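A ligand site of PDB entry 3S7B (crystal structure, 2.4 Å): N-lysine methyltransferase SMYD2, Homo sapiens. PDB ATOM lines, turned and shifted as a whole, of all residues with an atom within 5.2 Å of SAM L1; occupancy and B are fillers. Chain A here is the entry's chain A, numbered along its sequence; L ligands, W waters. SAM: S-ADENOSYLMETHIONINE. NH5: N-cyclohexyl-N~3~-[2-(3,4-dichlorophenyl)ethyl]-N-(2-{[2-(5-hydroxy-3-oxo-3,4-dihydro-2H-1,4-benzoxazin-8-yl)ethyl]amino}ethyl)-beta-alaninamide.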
ATOM      1  N   GLY A  16      -7.853  -4.244  -8.022  1.00  0.00           N
ATOM      2  CA  GLY A  16      -9.283  -3.972  -8.129  1.00  0.00           C
ATOM      3  C   GLY A  16      -9.675  -2.527  -7.891  1.00  0.00           C
ATOM      4  O   GLY A  16     -10.882  -2.238  -7.829  1.00  0.00           O
ATOM      5  N   LYS A  17      -8.691  -1.606  -7.726  1.00  0.00           N
ATOM      6  CA  LYS A  17      -8.956  -0.182  -7.441  1.00  0.00           C
ATOM      7  C   LYS A  17      -8.088   0.757  -8.293  1.00  0.00           C
ATOM      8  O   LYS A  17      -7.922   1.916  -7.927  1.00  0.00           O
ATOM      9  CB  LYS A  17      -8.743   0.145  -5.937  1.00  0.00           C
ATOM     10  CG  LYS A  17      -9.569  -0.636  -4.951  1.00  0.00           C
ATOM     11  CD  LYS A  17      -9.275  -0.196  -3.524  1.00  0.00           C
ATOM     12  CE  LYS A  17      -9.811  -1.145  -2.484  1.00  0.00           C
ATOM     13  NZ  LYS A  17      -9.172  -2.467  -2.600  1.00  0.00           N
ATOM     14  N   GLY A  18      -7.591   0.262  -9.416  1.00  0.00           N
ATOM     15  CA  GLY A  18      -6.767   1.010 -10.373  1.00  0.00           C
ATOM     16  C   GLY A  18      -5.496   1.525  -9.729  1.00  0.00           C
ATOM     17  O   GLY A  18      -4.798   0.754  -9.072  1.00  0.00           O
ATOM     18  N   ARG A  19      -5.222   2.830  -9.874  1.00  0.00           N
ATOM     19  CA  ARG A  19      -4.034   3.432  -9.244  1.00  0.00           C
ATOM     20  C   ARG A  19      -4.422   3.979  -7.871  1.00  0.00           C
ATOM     21  O   ARG A  19      -5.540   4.451  -7.669  1.00  0.00           O
ATOM     22  CB  ARG A  19      -3.420   4.537 -10.115  1.00  0.00           C
ATOM     23  CG  ARG A  19      -2.983   4.049 -11.499  1.00  0.00           C
ATOM     24  CD  ARG A  19      -2.998   5.166 -12.528  1.00  0.00           C
ATOM     25  NE  ARG A  19      -4.316   5.805 -12.651  1.00  0.00           N
ATOM     26  CZ  ARG A  19      -4.639   6.697 -13.585  1.00  0.00           C
ATOM     27  NH1 ARG A  19      -5.863   7.215 -13.616  1.00  0.00           N
ATOM     28  NH2 ARG A  19      -3.754   7.082 -14.489  1.00  0.00           N
ATOM     29  N   GLY A  20      -3.489   3.906  -6.955  1.00  0.00           N
ATOM     30  CA  GLY A  20      -3.694   4.390  -5.614  1.00  0.00           C
ATOM     31  C   GLY A  20      -2.446   4.987  -4.993  1.00  0.00           C
ATOM     32  O   GLY A  20      -1.374   5.019  -5.614  1.00  0.00           O
ATOM     33  N   LEU A 129       0.074  12.198  -9.968  1.00  0.00           N
ATOM     34  CA  LEU A 129      -0.986  11.949 -10.954  1.00  0.00           C
ATOM     35  C   LEU A 129      -1.246  13.242 -11.705  1.00  0.00           C
ATOM     36  O   LEU A 129      -1.356  14.306 -11.094  1.00  0.00           O
ATOM     37  CB  LEU A 129      -2.267  11.451 -10.239  1.00  0.00           C
ATOM     38  CG  LEU A 129      -3.478  11.085 -11.110  1.00  0.00           C
ATOM     39  CD1 LEU A 129      -3.209   9.838 -11.946  1.00  0.00           C
ATOM     40  CD2 LEU A 129      -4.728  10.903 -10.252  1.00  0.00           C
ATOM     41  N   GLU A 135      -8.935   9.220 -14.504  1.00  0.00           N
ATOM     42  CA  GLU A 135      -9.919   8.205 -14.843  1.00  0.00           C
ATOM     43  C   GLU A 135     -11.237   8.923 -15.182  1.00  0.00           C
ATOM     44  O   GLU A 135     -11.643   9.853 -14.486  1.00  0.00           O
ATOM     45  CB  GLU A 135     -10.124   7.245 -13.671  1.00  0.00           C
ATOM     46  CG  GLU A 135     -11.135   6.154 -13.971  1.00  0.00           C
ATOM     47  CD  GLU A 135     -11.009   4.935 -13.084  1.00  0.00           C
ATOM     48  OE1 GLU A 135     -10.983   3.817 -13.633  1.00  0.00           O
ATOM     49  OE2 GLU A 135     -10.925   5.095 -11.853  1.00  0.00           O
ATOM     50  N   HIS A 137     -14.234   6.964 -16.807  1.00  0.00           N
ATOM     51  CA  HIS A 137     -15.383   6.049 -16.861  1.00  0.00           C
ATOM     52  C   HIS A 137     -16.283   6.364 -18.062  1.00  0.00           C
ATOM     53  O   HIS A 137     -17.480   6.106 -18.024  1.00  0.00           O
ATOM     54  CB  HIS A 137     -16.176   6.037 -15.534  1.00  0.00           C
ATOM     55  CG  HIS A 137     -15.430   5.383 -14.430  1.00  0.00           C
ATOM     56  ND1 HIS A 137     -15.125   6.055 -13.280  1.00  0.00           N
ATOM     57  CD2 HIS A 137     -14.869   4.155 -14.391  1.00  0.00           C
ATOM     58  CE1 HIS A 137     -14.415   5.205 -12.565  1.00  0.00           C
ATOM     59  NE2 HIS A 137     -14.234   4.053 -13.196  1.00  0.00           N
ATOM     60  N   CYS A 181     -15.444  12.662 -11.870  1.00  0.00           N
ATOM     61  CA  CYS A 181     -14.758  11.581 -11.181  1.00  0.00           C
ATOM     62  C   CYS A 181     -13.712  12.046 -10.174  1.00  0.00           C
ATOM     63  O   CYS A 181     -13.494  11.388  -9.153  1.00  0.00           O
ATOM     64  CB  CYS A 181     -14.142  10.622 -12.207  1.00  0.00           C
ATOM     65  SG  CYS A 181     -13.414   9.126 -11.498  1.00  0.00           S
ATOM     66  N   ASN A 182     -13.034  13.178 -10.488  1.00  0.00           N
ATOM     67  CA  ASN A 182     -11.895  13.661  -9.740  1.00  0.00           C
ATOM     68  C   ASN A 182     -11.991  15.021  -9.076  1.00  0.00           C
ATOM     69  O   ASN A 182     -11.066  15.389  -8.331  1.00  0.00           O
ATOM     70  CB  ASN A 182     -10.632  13.563 -10.624  1.00  0.00           C
ATOM     71  CG  ASN A 182     -10.358  12.166 -11.115  1.00  0.00           C
ATOM     72  OD1 ASN A 182      -9.756  11.358 -10.419  1.00  0.00           O
ATOM     73  ND2 ASN A 182     -10.878  11.830 -12.277  1.00  0.00           N
ATOM     74  N   ALA A 203      -6.527  13.433  -5.789  1.00  0.00           N
ATOM     75  CA  ALA A 203      -7.457  12.562  -6.524  1.00  0.00           C
ATOM     76  C   ALA A 203      -6.891  11.154  -6.783  1.00  0.00           C
ATOM     77  O   ALA A 203      -7.649  10.253  -7.154  1.00  0.00           O
ATOM     78  CB  ALA A 203      -7.912  13.219  -7.821  1.00  0.00           C
ATOM     79  N   LEU A 204      -5.573  10.949  -6.519  1.00  0.00           N
ATOM     80  CA  LEU A 204      -4.956   9.647  -6.620  1.00  0.00           C
ATOM     81  C   LEU A 204      -5.513   8.719  -5.538  1.00  0.00           C
ATOM     82  O   LEU A 204      -5.594   7.506  -5.770  1.00  0.00           O
ATOM     83  CB  LEU A 204      -3.412   9.712  -6.549  1.00  0.00           C
ATOM     84  CG  LEU A 204      -2.613   8.378  -6.633  1.00  0.00           C
ATOM     85  CD1 LEU A 204      -2.964   7.590  -7.877  1.00  0.00           C
ATOM     86  CD2 LEU A 204      -1.132   8.632  -6.602  1.00  0.00           C
ATOM     87  N   MET A 205      -5.911   9.271  -4.384  1.00  0.00           N
ATOM     88  CA  MET A 205      -6.429   8.450  -3.285  1.00  0.00           C
ATOM     89  C   MET A 205      -7.755   7.792  -3.562  1.00  0.00           C
ATOM     90  O   MET A 205      -8.701   8.440  -4.016  1.00  0.00           O
ATOM     91  CB  MET A 205      -6.468   9.210  -1.951  1.00  0.00           C
ATOM     92  CG  MET A 205      -5.111   9.688  -1.485  1.00  0.00           C
ATOM     93  SD  MET A 205      -5.209  10.532   0.103  1.00  0.00           S
ATOM     94  CE  MET A 205      -6.006  12.117  -0.380  1.00  0.00           C
ATOM     95  N   ASN A 206      -7.819   6.504  -3.240  1.00  0.00           N
ATOM     96  CA  ASN A 206      -9.014   5.690  -3.359  1.00  0.00           C
ATOM     97  C   ASN A 206      -9.932   5.886  -2.163  1.00  0.00           C
ATOM     98  O   ASN A 206      -9.555   6.535  -1.178  1.00  0.00           O
ATOM     99  CB  ASN A 206      -8.649   4.214  -3.567  1.00  0.00           C
ATOM    100  CG  ASN A 206      -8.202   3.939  -4.959  1.00  0.00           C
ATOM    101  OD1 ASN A 206      -8.735   4.488  -5.917  1.00  0.00           O
ATOM    102  ND2 ASN A 206      -7.204   3.091  -5.116  1.00  0.00           N
ATOM    103  N   HIS A 207     -11.163   5.370  -2.285  1.00  0.00           N
ATOM    104  CA  HIS A 207     -12.202   5.501  -1.260  1.00  0.00           C
ATOM    105  C   HIS A 207     -12.268   4.319  -0.297  1.00  0.00           C
ATOM    106  O   HIS A 207     -12.077   3.164  -0.681  1.00  0.00           O
ATOM    107  CB  HIS A 207     -13.578   5.638  -1.931  1.00  0.00           C
ATOM    108  CG  HIS A 207     -14.705   5.601  -0.940  1.00  0.00           C
ATOM    109  ND1 HIS A 207     -15.314   4.396  -0.568  1.00  0.00           N
ATOM    110  CD2 HIS A 207     -15.241   6.594  -0.207  1.00  0.00           C
ATOM    111  CE1 HIS A 207     -16.191   4.719   0.375  1.00  0.00           C
ATOM    112  NE2 HIS A 207     -16.184   6.031   0.605  1.00  0.00           N
ATOM    113  N   SER A 208     -12.635   4.610   0.936  1.00  0.00           N
ATOM    114  CA  SER A 208     -12.995   3.652   1.978  1.00  0.00           C
ATOM    115  C   SER A 208     -14.043   4.300   2.872  1.00  0.00           C
ATOM    116  O   SER A 208     -13.987   5.516   3.091  1.00  0.00           O
ATOM    117  CB  SER A 208     -11.807   3.230   2.827  1.00  0.00           C
ATOM    118  OG  SER A 208     -12.238   2.360   3.861  1.00  0.00           O
ATOM    119  N   PHE A 237      -6.515   5.917   2.163  1.00  0.00           N
ATOM    120  CA  PHE A 237      -7.919   6.066   1.769  1.00  0.00           C
ATOM    121  C   PHE A 237      -8.588   7.242   2.428  1.00  0.00           C
ATOM    122  O   PHE A 237      -8.449   7.483   3.626  1.00  0.00           O
ATOM    123  CB  PHE A 237      -8.749   4.815   2.127  1.00  0.00           C
ATOM    124  CG  PHE A 237      -8.374   3.507   1.474  1.00  0.00           C
ATOM    125  CD1 PHE A 237      -8.659   3.279   0.132  1.00  0.00           C
ATOM    126  CD2 PHE A 237      -7.808   2.485   2.229  1.00  0.00           C
ATOM    127  CE1 PHE A 237      -8.354   2.043  -0.458  1.00  0.00           C
ATOM    128  CE2 PHE A 237      -7.491   1.248   1.632  1.00  0.00           C
ATOM    129  CZ  PHE A 237      -7.749   1.052   0.287  1.00  0.00           C
ATOM    130  N   TYR A 240     -15.146   9.440  -0.018  1.00  0.00           N
ATOM    131  CA  TYR A 240     -15.691  10.269  -1.099  1.00  0.00           C
ATOM    132  C   TYR A 240     -17.117  10.749  -0.760  1.00  0.00           C
ATOM    133  O   TYR A 240     -17.635  11.625  -1.440  1.00  0.00           O
ATOM    134  CB  TYR A 240     -15.803   9.424  -2.404  1.00  0.00           C
ATOM    135  CG  TYR A 240     -14.521   9.007  -3.094  1.00  0.00           C
ATOM    136  CD1 TYR A 240     -13.261   9.276  -2.533  1.00  0.00           C
ATOM    137  CD2 TYR A 240     -14.543   8.315  -4.308  1.00  0.00           C
ATOM    138  CE1 TYR A 240     -12.081   8.848  -3.141  1.00  0.00           C
ATOM    139  CE2 TYR A 240     -13.373   7.921  -4.953  1.00  0.00           C
ATOM    140  CZ  TYR A 240     -12.138   8.176  -4.348  1.00  0.00           C
ATOM    141  OH  TYR A 240     -10.980   7.829  -4.994  1.00  0.00           O
ATOM    142  N   TYR A 258     -19.353   7.298  -8.841  1.00  0.00           N
ATOM    143  CA  TYR A 258     -17.977   6.805  -9.015  1.00  0.00           C
ATOM    144  C   TYR A 258     -17.817   5.474  -9.689  1.00  0.00           C
ATOM    145  O   TYR A 258     -16.687   5.031  -9.864  1.00  0.00           O
ATOM    146  CB  TYR A 258     -17.164   6.931  -7.706  1.00  0.00           C
ATOM    147  CG  TYR A 258     -17.108   8.348  -7.197  1.00  0.00           C
ATOM    148  CD1 TYR A 258     -16.294   9.300  -7.814  1.00  0.00           C
ATOM    149  CD2 TYR A 258     -17.936   8.775  -6.153  1.00  0.00           C
ATOM    150  CE1 TYR A 258     -16.296  10.632  -7.385  1.00  0.00           C
ATOM    151  CE2 TYR A 258     -17.956  10.102  -5.738  1.00  0.00           C
ATOM    152  CZ  TYR A 258     -17.136  11.031  -6.354  1.00  0.00           C
ATOM    153  OH  TYR A 258     -17.166  12.330  -5.938  1.00  0.00           O
ATOM    154  N   PHE A 259     -18.922   4.861 -10.116  1.00  0.00           N
ATOM    155  CA  PHE A 259     -18.947   3.605 -10.900  1.00  0.00           C
ATOM    156  C   PHE A 259     -18.235   2.415 -10.257  1.00  0.00           C
ATOM    157  O   PHE A 259     -17.613   1.619 -10.950  1.00  0.00           O
ATOM    158  CB  PHE A 259     -18.471   3.848 -12.345  1.00  0.00           C
ATOM    159  CG  PHE A 259     -19.110   5.030 -13.018  1.00  0.00           C
ATOM    160  CD1 PHE A 259     -20.283   4.881 -13.770  1.00  0.00           C
ATOM    161  CD2 PHE A 259     -18.530   6.295 -12.944  1.00  0.00           C
ATOM    162  CE1 PHE A 259     -20.871   5.984 -14.413  1.00  0.00           C
ATOM    163  CE2 PHE A 259     -19.118   7.399 -13.588  1.00  0.00           C
ATOM    164  CZ  PHE A 259     -20.282   7.243 -14.311  1.00  0.00           C
ATOM    165  N   PHE A 260     -18.320   2.298  -8.927  1.00  0.00           N
ATOM    166  CA  PHE A 260     -17.719   1.178  -8.220  1.00  0.00           C
ATOM    167  C   PHE A 260     -18.516   0.850  -6.981  1.00  0.00           C
ATOM    168  O   PHE A 260     -19.263   1.685  -6.471  1.00  0.00           O
ATOM    169  CB  PHE A 260     -16.226   1.460  -7.865  1.00  0.00           C
ATOM    170  CG  PHE A 260     -16.001   2.315  -6.648  1.00  0.00           C
ATOM    171  CD1 PHE A 260     -15.839   1.745  -5.395  1.00  0.00           C
ATOM    172  CD2 PHE A 260     -15.922   3.714  -6.748  1.00  0.00           C
ATOM    173  CE1 PHE A 260     -15.654   2.537  -4.245  1.00  0.00           C
ATOM    174  CE2 PHE A 260     -15.717   4.516  -5.607  1.00  0.00           C
ATOM    175  CZ  PHE A 260     -15.585   3.924  -4.373  1.00  0.00           C
ATOM    176  N   THR A 261     -18.332  -0.376  -6.485  1.00  0.00           N
ATOM    177  CA  THR A 261     -18.896  -0.863  -5.233  1.00  0.00           C
ATOM    178  C   THR A 261     -17.731  -1.017  -4.265  1.00  0.00           C
ATOM    179  O   THR A 261     -16.715  -1.643  -4.607  1.00  0.00           O
ATOM    180  CB  THR A 261     -19.685  -2.172  -5.433  1.00  0.00           C
ATOM    181  OG1 THR A 261     -20.775  -1.945  -6.307  1.00  0.00           O
ATOM    182  CG2 THR A 261     -20.203  -2.759  -4.130  1.00  0.00           C
ATOM    183  N   CYS A 262     -17.883  -0.439  -3.070  1.00  0.00           N
ATOM    184  CA  CYS A 262     -16.901  -0.516  -2.007  1.00  0.00           C
ATOM    185  C   CYS A 262     -17.000  -1.863  -1.328  1.00  0.00           C
ATOM    186  O   CYS A 262     -18.091  -2.383  -1.086  1.00  0.00           O
ATOM    187  CB  CYS A 262     -17.101   0.627  -1.014  1.00  0.00           C
ATOM    188  SG  CYS A 262     -15.828   0.708   0.289  1.00  0.00           S
HETATM  189  N   SAM L   1      -8.048   4.626  -8.626  1.00  0.00           N
HETATM  190  CA  SAM L   1      -8.159   5.955  -9.319  1.00  0.00           C
HETATM  191  C   SAM L   1      -7.266   6.055 -10.553  1.00  0.00           C
HETATM  192  O   SAM L   1      -7.197   7.116 -11.165  1.00  0.00           O
HETATM  193  OXT SAM L   1      -6.626   5.076 -10.942  1.00  0.00           O
HETATM  194  CB  SAM L   1      -7.865   7.126  -8.342  1.00  0.00           C
HETATM  195  CG  SAM L   1      -9.121   7.574  -7.533  1.00  0.00           C
HETATM  196  SD  SAM L   1     -10.321   8.386  -8.672  1.00  0.00           S
HETATM  197  CE  SAM L   1     -10.719   9.931  -7.934  1.00  0.00           C
HETATM  198  C5' SAM L   1     -11.896   7.601  -8.385  1.00  0.00           C
HETATM  199  C4' SAM L   1     -11.960   6.206  -9.085  1.00  0.00           C
HETATM  200  O4' SAM L   1     -11.107   5.230  -8.454  1.00  0.00           O
HETATM  201  C3' SAM L   1     -13.368   5.635  -8.902  1.00  0.00           C
HETATM  202  O3' SAM L   1     -14.325   6.176  -9.777  1.00  0.00           O
HETATM  203  C2' SAM L   1     -13.143   4.116  -9.020  1.00  0.00           C
HETATM  204  O2' SAM L   1     -12.936   3.712 -10.385  1.00  0.00           O
HETATM  205  C1' SAM L   1     -11.811   3.974  -8.269  1.00  0.00           C
HETATM  206  N9  SAM L   1     -11.940   3.678  -6.847  1.00  0.00           N
HETATM  207  C8  SAM L   1     -11.761   4.573  -5.764  1.00  0.00           C
HETATM  208  N7  SAM L   1     -11.951   3.910  -4.674  1.00  0.00           N
HETATM  209  C5  SAM L   1     -12.271   2.599  -4.952  1.00  0.00           C
HETATM  210  C6  SAM L   1     -12.569   1.435  -4.181  1.00  0.00           C
HETATM  211  N6  SAM L   1     -12.595   1.464  -2.822  1.00  0.00           N
HETATM  212  N1  SAM L   1     -12.877   0.247  -4.867  1.00  0.00           N
HETATM  213  C2  SAM L   1     -12.884   0.180  -6.230  1.00  0.00           C
HETATM  214  N3  SAM L   1     -12.576   1.246  -6.970  1.00  0.00           N
HETATM  215  C4  SAM L   1     -12.257   2.447  -6.377  1.00  0.00           C
HETATM  216  C1  NH5 L   2     -21.132  11.262 -11.975  1.00  0.00           C
HETATM  217  C2  NH5 L   2     -20.381  11.115 -13.139  1.00  0.00           C
HETATM  218  C3  NH5 L   2     -20.740  11.840 -14.279  1.00  0.00           C
HETATM  219  C4  NH5 L   2     -21.838  12.710 -14.247  1.00  0.00           C
HETATM  220  C5  NH5 L   2     -22.576  12.855 -13.076  1.00  0.00           C
HETATM  221  C6  NH5 L   2     -22.226  12.120 -11.936  1.00  0.00           C
HETATM  222  C7  NH5 L   2     -23.041  12.253 -10.670  1.00  0.00           C
HETATM  223  C8  NH5 L   2     -22.638  13.429  -9.774  1.00  0.00           C
HETATM  224  N9  NH5 L   2     -21.309  13.984 -10.109  1.00  0.00           N
HETATM  225  C10 NH5 L   2     -20.378  13.814  -8.992  1.00  0.00           C
HETATM  226  C11 NH5 L   2     -19.484  15.063  -8.935  1.00  0.00           C
HETATM  227  C12 NH5 L   2     -19.280  15.551  -7.500  1.00  0.00           C
HETATM  228  O13 NH5 L   2     -19.684  14.883  -6.565  1.00  0.00           O
HETATM  229  N14 NH5 L   2     -18.615  16.714  -7.298  1.00  0.00           N
HETATM  230  C15 NH5 L   2     -18.398  17.296  -5.965  1.00  0.00           C
HETATM  231  C16 NH5 L   2     -17.942  16.283  -4.904  1.00  0.00           C
HETATM  232  N17 NH5 L   2     -16.487  16.086  -4.892  1.00  0.00           N
HETATM  233  C18 NH5 L   2     -16.055  15.542  -3.584  1.00  0.00           C
HETATM  234  C19 NH5 L   2     -16.079  14.006  -3.452  1.00  0.00           C
HETATM  235  C20 NH5 L   2     -14.724  13.534  -2.974  1.00  0.00           C
HETATM  236  C21 NH5 L   2     -14.352  13.616  -1.615  1.00  0.00           C
HETATM  237  C22 NH5 L   2     -13.093  13.186  -1.165  1.00  0.00           C
HETATM  238  C23 NH5 L   2     -12.173  12.697  -2.103  1.00  0.00           C
HETATM  239  C24 NH5 L   2     -12.550  12.592  -3.440  1.00  0.00           C
HETATM  240  C25 NH5 L   2     -13.787  13.034  -3.856  1.00  0.00           C
HETATM  241  O26 NH5 L   2     -14.094  13.028  -5.178  1.00  0.00           O
HETATM  242  C27 NH5 L   2     -13.009  13.310  -6.091  1.00  0.00           C
HETATM  243  C28 NH5 L   2     -11.741  12.580  -5.708  1.00  0.00           C
HETATM  244  O29 NH5 L   2     -10.884  12.310  -6.517  1.00  0.00           O
HETATM  245  N30 NH5 L   2     -11.615  12.246  -4.419  1.00  0.00           N
HETATM  246  O31 NH5 L   2     -10.904  12.294  -1.816  1.00  0.00           O
HETATM  247  C32 NH5 L   2     -18.154  17.543  -8.452  1.00  0.00           C
HETATM  248  C33 NH5 L   2     -19.199  18.632  -8.818  1.00  0.00           C
HETATM  249  C34 NH5 L   2     -18.759  19.467 -10.021  1.00  0.00           C
HETATM  250  C35 NH5 L   2     -17.368  20.095  -9.795  1.00  0.00           C
HETATM  251  C36 NH5 L   2     -16.301  19.033  -9.437  1.00  0.00           C
HETATM  252  C37 NH5 L   2     -16.753  18.152  -8.260  1.00  0.00           C
HETATM  253 CL38 NH5 L   2     -22.311  13.625 -15.658  1.00  0.00          CL
HETATM  254 CL39 NH5 L   2     -19.795  11.707 -15.726  1.00  0.00          CL
HETATM  255  O   HOH W   1      -8.070   9.528 -11.724  1.00  0.00           O
HETATM  256  O   HOH W   2     -13.361  -1.203  -1.426  1.00  0.00           O
HETATM  257  O   HOH W   3     -13.940  -2.104  -4.060  1.00  0.00           O
HETATM  258  O   HOH W   4     -12.235   0.598   0.276  1.00  0.00           O
HETATM  259  O   HOH W   5      -9.381   3.200 -10.553  1.00  0.00           O
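O3' of SAM L1 is in hydrogen-bond range of O of Tyr 258 (2.6 Å). The backbone NH of Arg 19 lies within hydrogen-bond range of an oxygen (OXT) of SAM L1 (2.9 Å). O of Arg 19 is in hydrogen-bond range of N of SAM L1 (2.7 Å). An oxygen (O) of SAM L1 is in salt-bridge range of the guanidinium group (NH1) of Arg 19, at 2.8 Å. N7 of SAM L1 lies within hydrogen-bond range of N of His 207 (2.9 Å). O of His 207 is in hydrogen-bond range of N6 of SAM L1. OD1 of Asn 206 sits at hydrogen-bond distance from N of SAM L1, 2.8 Å away. The backbone carbonyl oxygen of Lys 17 sits at hydrogen-bond distance from a nitrogen (N) of SAM L1, at 2.8 Å. O2' of SAM L1 sits at hydrogen-bond distance from OE2 of Glu 135 (2.8 Å). An oxygen (O2') of SAM L1 sits close to a ring nitrogen (NE2) of His 137 (3.1 Å). SG of Cys 181 is in hydrogen-bond range of O3' of SAM L1, 3.5 Å away. O26 of NH5 L2 lies close to OH of Tyr 258, at 3.2 Å.
Water W1 lies within hydrogen-bond range of O of SAM L1 (2.6 Å), OD1 of Asn 182 (2.8 Å) and N of Glu 135 (2.9 Å). Water W3 bridges a nitrogen (N1) of SAM L1 and the backbone carbonyl oxygen of Thr 261. Water W5 lies within hydrogen-bond range of N of SAM L1 (2.7 Å), OE2 of Glu 135 (2.8 Å) and O of Lys 17 (3.3 Å). Water W4 lies within hydrogen-bond range of the backbone carbonyl oxygen of His 207 and a nitrogen (N6) of SAM L1.
The backbone carbonyl oxygen (O) of Arg 19 lies within hydrogen-bond range of the side-chain amide nitrogen (ND2) of Asn 206 (3.3 Å). The side-chain amide nitrogen (ND2) of Asn 206 is in hydrogen-bond range of the backbone carbonyl oxygen (O) of Lys 17 (3.1 Å). The side-chain carboxylate (OE1) of Glu 135 sits at hydrogen-bond distance from a ring nitrogen (NE2) of His 137. The side-chain amide nitrogen of Asn 182 lies within hydrogen-bond range of the backbone carbonyl oxygen of Glu 135 (3.1 Å). The side-chain sulfur (SG) of Cys 181 lies close to the backbone carbonyl oxygen (O) of Glu 135 (3.5 Å). The side-chain amide nitrogen of Asn 182 sits close to the side-chain sulfur of Cys 181 (3.8 Å). The backbone carbonyl oxygen of Met 205 lies within hydrogen-bond range of the side-chain hydroxyl of Tyr 240, at 2.6 Å.
A sulfur (SD) of SAM L1 sits close to the side-chain amide oxygen (OD1) of Asn 182 (3.5 Å). A sulfur (SD) of SAM L1 sits close to the backbone carbonyl oxygen (O) of Ala 203 (3.6 Å). The side-chain hydroxyl (OH) of Tyr 240 sits close to a sulfur (SD) of SAM L1, at 3.8 Å. Gly 16 touches SAM L1 (O to C2, 3.5 Å). C of Gly 18 touches OXT of SAM L1 (3.9 Å). Leu 204 touches SAM L1. O of Met 205 touches CG of SAM L1, at 3.6 Å. Phe 260 touches SAM L1 (CE1 to C6, 3.3 Å). Hydrophobic or aromatic side chains that line SAM L1: His 137, His 207, Tyr 240, Tyr 258 and Phe 260. 16 residues have an atom within 4 Å of SAM L1: Gly 16, Lys 17, Gly 18, Arg 19, Glu 135, His 137, Cys 181, Asn 182, Ala 203, Leu 204, Met 205, Asn 206, His 207, Tyr 240, Tyr 258 and Phe 260. Along chain A the residues within 4 Å of SAM L1 span positions 16 to 260.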
